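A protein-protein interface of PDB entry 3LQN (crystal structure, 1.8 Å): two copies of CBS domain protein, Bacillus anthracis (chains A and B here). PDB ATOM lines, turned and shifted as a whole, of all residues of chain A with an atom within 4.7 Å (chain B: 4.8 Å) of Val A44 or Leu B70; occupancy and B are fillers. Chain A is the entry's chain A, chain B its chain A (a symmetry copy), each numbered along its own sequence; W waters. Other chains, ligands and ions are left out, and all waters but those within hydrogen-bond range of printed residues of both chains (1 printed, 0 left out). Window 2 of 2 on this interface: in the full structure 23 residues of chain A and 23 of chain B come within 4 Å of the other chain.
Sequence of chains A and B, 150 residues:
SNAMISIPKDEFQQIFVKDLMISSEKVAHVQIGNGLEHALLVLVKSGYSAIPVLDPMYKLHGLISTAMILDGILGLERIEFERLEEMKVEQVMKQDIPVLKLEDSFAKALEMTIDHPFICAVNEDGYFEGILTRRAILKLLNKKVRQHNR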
ATOM      1  N   LEU A  40      21.410  -0.195 -30.811  1.00  0.00           N
ATOM      2  CA  LEU A  40      22.560   0.654 -30.508  1.00  0.00           C
ATOM      3  C   LEU A  40      22.845   0.607 -29.008  1.00  0.00           C
ATOM      4  O   LEU A  40      24.008   0.579 -28.569  1.00  0.00           O
ATOM      5  CB  LEU A  40      22.299   2.091 -30.996  1.00  0.00           C
ATOM      6  CG  LEU A  40      23.512   3.001 -30.791  1.00  0.00           C
ATOM      7  CD1 LEU A  40      24.708   2.591 -31.738  1.00  0.00           C
ATOM      8  CD2 LEU A  40      23.077   4.437 -31.149  1.00  0.00           C
ATOM      9  N   LEU A  41      21.784   0.539 -28.198  1.00  0.00           N
ATOM     10  CA  LEU A  41      22.016   0.450 -26.764  1.00  0.00           C
ATOM     11  C   LEU A  41      22.695  -0.874 -26.363  1.00  0.00           C
ATOM     12  O   LEU A  41      23.575  -0.904 -25.496  1.00  0.00           O
ATOM     13  CB  LEU A  41      20.661   0.630 -26.024  1.00  0.00           C
ATOM     14  CG  LEU A  41      20.707   0.858 -24.521  1.00  0.00           C
ATOM     15  CD1 LEU A  41      21.480   2.107 -24.156  1.00  0.00           C
ATOM     16  CD2 LEU A  41      19.250   0.952 -23.992  1.00  0.00           C
ATOM     17  N   VAL A  42      22.280  -1.958 -26.998  1.00  0.00           N
ATOM     18  CA  VAL A  42      22.847  -3.263 -26.723  1.00  0.00           C
ATOM     19  C   VAL A  42      24.332  -3.254 -27.112  1.00  0.00           C
ATOM     20  O   VAL A  42      25.174  -3.727 -26.315  1.00  0.00           O
ATOM     21  CB  VAL A  42      22.095  -4.372 -27.461  1.00  0.00           C
ATOM     22  CG1 VAL A  42      22.878  -5.754 -27.416  1.00  0.00           C
ATOM     23  CG2 VAL A  42      20.668  -4.553 -26.880  1.00  0.00           C
ATOM     24  N   LEU A  43      24.638  -2.674 -28.283  1.00  0.00           N
ATOM     25  CA  LEU A  43      26.044  -2.523 -28.730  1.00  0.00           C
ATOM     26  C   LEU A  43      26.866  -1.732 -27.728  1.00  0.00           C
ATOM     27  O   LEU A  43      27.931  -2.155 -27.289  1.00  0.00           O
ATOM     28  CB  LEU A  43      26.119  -1.856 -30.138  1.00  0.00           C
ATOM     29  CG  LEU A  43      25.851  -2.860 -31.220  1.00  0.00           C
ATOM     30  CD1 LEU A  43      25.370  -2.048 -32.401  1.00  0.00           C
ATOM     31  CD2 LEU A  43      27.221  -3.568 -31.533  1.00  0.00           C
ATOM     32  N   VAL A  44      26.343  -0.587 -27.311  1.00  0.00           N
ATOM     33  CA  VAL A  44      27.118   0.268 -26.427  1.00  0.00           C
ATOM     34  C   VAL A  44      27.269  -0.349 -25.051  1.00  0.00           C
ATOM     35  O   VAL A  44      28.352  -0.275 -24.438  1.00  0.00           O
ATOM     36  CB  VAL A  44      26.489   1.673 -26.305  1.00  0.00           C
ATOM     37  CG1 VAL A  44      27.230   2.566 -25.237  1.00  0.00           C
ATOM     38  CG2 VAL A  44      26.469   2.387 -27.674  1.00  0.00           C
ATOM     39  N   LYS A  45      26.167  -0.893 -24.525  1.00  0.00           N
ATOM     40  CA  LYS A  45      26.175  -1.500 -23.189  1.00  0.00           C
ATOM     41  C   LYS A  45      27.080  -2.717 -23.106  1.00  0.00           C
ATOM     42  O   LYS A  45      27.724  -2.946 -22.064  1.00  0.00           O
ATOM     43  CB  LYS A  45      24.768  -1.834 -22.698  1.00  0.00           C
ATOM     44  CG  LYS A  45      23.975  -0.587 -22.288  1.00  0.00           C
ATOM     45  CD  LYS A  45      22.597  -0.982 -21.705  1.00  0.00           C
ATOM     46  CE  LYS A  45      22.782  -1.692 -20.387  1.00  0.00           C
ATOM     47  NZ  LYS A  45      21.507  -2.301 -19.915  1.00  0.00           N
ATOM     48  N   SER A  46      27.189  -3.452 -24.208  1.00  0.00           N
ATOM     49  CA  SER A  46      27.970  -4.685 -24.218  1.00  0.00           C
ATOM     50  C   SER A  46      29.459  -4.420 -24.414  1.00  0.00           C
ATOM     51  O   SER A  46      30.282  -5.187 -23.970  1.00  0.00           O
ATOM     52  CB  SER A  46      27.465  -5.624 -25.309  1.00  0.00           C
ATOM     53  OG  SER A  46      27.878  -5.224 -26.583  1.00  0.00           O
ATOM     54  N   GLY A  47      29.785  -3.294 -25.038  1.00  0.00           N
ATOM     55  CA  GLY A  47      31.167  -2.974 -25.358  1.00  0.00           C
ATOM     56  C   GLY A  47      31.674  -3.647 -26.625  1.00  0.00           C
ATOM     57  O   GLY A  47      32.847  -3.522 -26.947  1.00  0.00           O
ATOM     58  N   THR A  66      28.054  -0.629 -34.723  1.00  0.00           N
ATOM     59  CA  THR A  66      27.766   0.752 -34.437  1.00  0.00           C
ATOM     60  C   THR A  66      28.046   1.612 -35.665  1.00  0.00           C
ATOM     61  O   THR A  66      27.341   2.594 -35.919  1.00  0.00           O
ATOM     62  CB  THR A  66      28.598   1.235 -33.232  1.00  0.00           C
ATOM     63  OG1 THR A  66      28.324   0.370 -32.121  1.00  0.00           O
ATOM     64  CG2 THR A  66      28.248   2.673 -32.870  1.00  0.00           C
ATOM     65  N   LEU A  70      25.273   4.151 -37.328  1.00  0.00           N
ATOM     66  CA  LEU A  70      25.544   5.588 -37.520  1.00  0.00           C
ATOM     67  C   LEU A  70      25.574   5.952 -39.041  1.00  0.00           C
ATOM     68  O   LEU A  70      25.043   6.971 -39.440  1.00  0.00           O
ATOM     69  CB  LEU A  70      26.856   5.977 -36.847  1.00  0.00           C
ATOM     70  CG  LEU A  70      26.817   5.719 -35.328  1.00  0.00           C
ATOM     71  CD1 LEU A  70      28.225   6.031 -34.741  1.00  0.00           C
ATOM     72  CD2 LEU A  70      25.702   6.574 -34.673  1.00  0.00           C
ATOM     73  N   THR B  66      34.366   6.356 -31.585  1.00  0.00           N
ATOM     74  CA  THR B  66      32.927   6.392 -31.552  1.00  0.00           C
ATOM     75  C   THR B  66      32.414   5.723 -30.281  1.00  0.00           C
ATOM     76  O   THR B  66      31.405   6.147 -29.709  1.00  0.00           O
ATOM     77  CB  THR B  66      32.344   5.704 -32.802  1.00  0.00           C
ATOM     78  OG1 THR B  66      32.888   6.348 -33.963  1.00  0.00           O
ATOM     79  CG2 THR B  66      30.824   5.801 -32.819  1.00  0.00           C
ATOM     80  N   ALA B  67      33.093   4.645 -29.865  1.00  0.00           N
ATOM     81  CA  ALA B  67      32.794   4.049 -28.578  1.00  0.00           C
ATOM     82  C   ALA B  67      32.892   5.087 -27.410  1.00  0.00           C
ATOM     83  O   ALA B  67      32.010   5.092 -26.526  1.00  0.00           O
ATOM     84  CB  ALA B  67      33.659   2.797 -28.326  1.00  0.00           C
ATOM     85  N   MET B  68      33.933   5.913 -27.359  1.00  0.00           N
ATOM     86  CA  MET B  68      34.144   6.844 -26.246  1.00  0.00           C
ATOM     87  C   MET B  68      33.014   7.889 -26.248  1.00  0.00           C
ATOM     88  O   MET B  68      32.454   8.234 -25.216  1.00  0.00           O
ATOM     89  CB  MET B  68      35.476   7.595 -26.329  1.00  0.00           C
ATOM     90  CG  MET B  68      36.670   6.723 -26.069  1.00  0.00           C
ATOM     91  SD  MET B  68      38.150   7.662 -26.420  1.00  0.00           S
ATOM     92  CE  MET B  68      39.183   6.351 -27.035  1.00  0.00           C
ATOM     93  N   ILE B  69      32.669   8.302 -27.451  1.00  0.00           N
ATOM     94  CA  ILE B  69      31.574   9.261 -27.589  1.00  0.00           C
ATOM     95  C   ILE B  69      30.235   8.728 -27.123  1.00  0.00           C
ATOM     96  O   ILE B  69      29.540   9.388 -26.313  1.00  0.00           O
ATOM     97  CB  ILE B  69      31.490   9.784 -29.023  1.00  0.00           C
ATOM     98  CG1 ILE B  69      32.785  10.587 -29.324  1.00  0.00           C
ATOM     99  CG2 ILE B  69      30.245  10.730 -29.148  1.00  0.00           C
ATOM    100  CD1 ILE B  69      32.813  11.162 -30.825  1.00  0.00           C
ATOM    101  N   LEU B  70      29.859   7.555 -27.632  1.00  0.00           N
ATOM    102  CA  LEU B  70      28.566   6.957 -27.251  1.00  0.00           C
ATOM    103  C   LEU B  70      28.551   6.580 -25.733  1.00  0.00           C
ATOM    104  O   LEU B  70      27.567   6.804 -25.054  1.00  0.00           O
ATOM    105  CB  LEU B  70      28.271   5.733 -28.112  1.00  0.00           C
ATOM    106  CG  LEU B  70      28.184   6.095 -29.608  1.00  0.00           C
ATOM    107  CD1 LEU B  70      27.997   4.780 -30.421  1.00  0.00           C
ATOM    108  CD2 LEU B  70      27.029   7.102 -29.843  1.00  0.00           C
ATOM    109  N   ASP B  71      29.679   6.112 -25.212  1.00  0.00           N
ATOM    110  CA  ASP B  71      29.762   5.787 -23.760  1.00  0.00           C
ATOM    111  C   ASP B  71      29.522   7.063 -22.941  1.00  0.00           C
ATOM    112  O   ASP B  71      28.962   7.044 -21.839  1.00  0.00           O
ATOM    113  CB  ASP B  71      31.163   5.261 -23.412  1.00  0.00           C
ATOM    114  CG  ASP B  71      31.363   3.818 -23.835  1.00  0.00           C
ATOM    115  OD1 ASP B  71      30.382   3.210 -24.274  1.00  0.00           O
ATOM    116  OD2 ASP B  71      32.484   3.302 -23.749  1.00  0.00           O
ATOM    117  N   GLY B  72      29.953   8.167 -23.496  1.00  0.00           N
ATOM    118  CA  GLY B  72      29.867   9.455 -22.850  1.00  0.00           C
ATOM    119  C   GLY B  72      28.450   9.947 -22.770  1.00  0.00           C
ATOM    120  O   GLY B  72      28.179  10.823 -21.979  1.00  0.00           O
ATOM    121  N   ILE B  73      27.555   9.414 -23.601  1.00  0.00           N
ATOM    122  CA  ILE B  73      26.154   9.799 -23.550  1.00  0.00           C
ATOM    123  C   ILE B  73      25.236   8.584 -23.274  1.00  0.00           C
ATOM    124  O   ILE B  73      24.074   8.560 -23.658  1.00  0.00           O
ATOM    125  CB  ILE B  73      25.689  10.510 -24.834  1.00  0.00           C
ATOM    126  CG1 ILE B  73      26.016   9.684 -26.060  1.00  0.00           C
ATOM    127  CG2 ILE B  73      26.347  11.881 -24.965  1.00  0.00           C
ATOM    128  CD1 ILE B  73      25.374  10.200 -27.330  1.00  0.00           C
ATOM    129  N   LEU B  74      25.777   7.597 -22.583  1.00  0.00           N
ATOM    130  CA  LEU B  74      25.008   6.387 -22.291  1.00  0.00           C
ATOM    131  C   LEU B  74      24.044   6.676 -21.116  1.00  0.00           C
ATOM    132  O   LEU B  74      24.467   6.803 -19.967  1.00  0.00           O
ATOM    133  CB  LEU B  74      25.917   5.238 -21.927  1.00  0.00           C
ATOM    134  CG  LEU B  74      25.208   3.956 -21.437  1.00  0.00           C
ATOM    135  CD1 LEU B  74      24.272   3.435 -22.517  1.00  0.00           C
ATOM    136  CD2 LEU B  74      26.158   2.889 -21.016  1.00  0.00           C
ATOM    137  N   ILE B  79      20.542   6.090 -25.564  1.00  0.00           N
ATOM    138  CA  ILE B  79      21.771   6.829 -25.849  1.00  0.00           C
ATOM    139  C   ILE B  79      21.318   8.273 -25.958  1.00  0.00           C
ATOM    140  O   ILE B  79      20.454   8.591 -26.786  1.00  0.00           O
ATOM    141  CB  ILE B  79      22.431   6.360 -27.149  1.00  0.00           C
ATOM    142  CG1 ILE B  79      22.862   4.864 -27.090  1.00  0.00           C
ATOM    143  CG2 ILE B  79      23.633   7.263 -27.477  1.00  0.00           C
ATOM    144  CD1 ILE B  79      23.976   4.470 -25.973  1.00  0.00           C
ATOM    145  N   PHE B  81      21.654  11.395 -27.182  1.00  0.00           N
ATOM    146  CA  PHE B  81      22.323  12.178 -28.224  1.00  0.00           C
ATOM    147  C   PHE B  81      22.152  13.706 -28.094  1.00  0.00           C
ATOM    148  O   PHE B  81      22.975  14.459 -28.601  1.00  0.00           O
ATOM    149  CB  PHE B  81      21.928  11.711 -29.639  1.00  0.00           C
ATOM    150  CG  PHE B  81      22.462  10.340 -30.000  1.00  0.00           C
ATOM    151  CD1 PHE B  81      23.820  10.122 -30.126  1.00  0.00           C
ATOM    152  CD2 PHE B  81      21.603   9.269 -30.176  1.00  0.00           C
ATOM    153  CE1 PHE B  81      24.306   8.858 -30.441  1.00  0.00           C
ATOM    154  CE2 PHE B  81      22.063   8.029 -30.491  1.00  0.00           C
ATOM    155  CZ  PHE B  81      23.421   7.811 -30.633  1.00  0.00           C
HETATM  156  O   HOH W   1      30.687   0.765 -25.412  1.00  0.00           O
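Thr A66 touches Leu B70, and with the chains exchanged Leu A70 touches Thr B66. Positions printed for both chains: 66 and 70. Of the 8 pairs that touch across the chains among the printed residues, 2 have their exchanged pair printed and touching as well.
Among the printed residues, merely in contact across the chains: Thr A66 with Leu B70 (3.2 Å), Leu A70 with Thr B66 (3.2 Å), Val A44 with Asp B71 (3.4 Å), Leu A40 with Phe B81 (3.4 Å), Leu A41 with Leu B74 (3.5 Å), Val A44 with Ile B79 (3.7 Å), Val A44 with Leu B70 (3.8 Å) and Leu A41 with Ile B79 (3.9 Å).
Water W1 bridges the side-chain carboxylate of Asp B71 (2.7 Å) and the backbone carbonyl oxygen of Val A44 (2.7 Å).
Of the printed residues of chain A, Leu B70 touches Val A44 and Thr A66. Printed residues of chain B within 4 Å of Leu A70: Thr B66. Printed residues of chain A within 4 Å of Asp B71: Val A44 (3.4 Å). Of the printed residues of chain B, Leu A41 touches Leu B74 and Ile B79. Printed residues of chain A within 4 Å of Ile B79: Leu A41 (3.9 Å) and Val A44 (3.7 Å). Of the printed residues of chain B, Thr A66 touches Leu B70 (3.2 Å). The nearest residue of chain B that does not touch Val A44 is Leu B74 (4.1 Å). The nearest printed residue of chain A that does not touch Leu B70 is Leu A40 (4.2 Å). The nearest printed residue of chain A that does not touch Ile B79 is Leu A40 (4.1 Å).
Hydrophobic or aromatic side chains of chain A within 4 Å of the printed part of chain B: Leu A40, Leu A41, Val A44 and Leu A70. Among the printed residues, no Asp or Glu carboxylate lies within 4 Å of a Lys or Arg side-chain nitrogen of the other chain.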
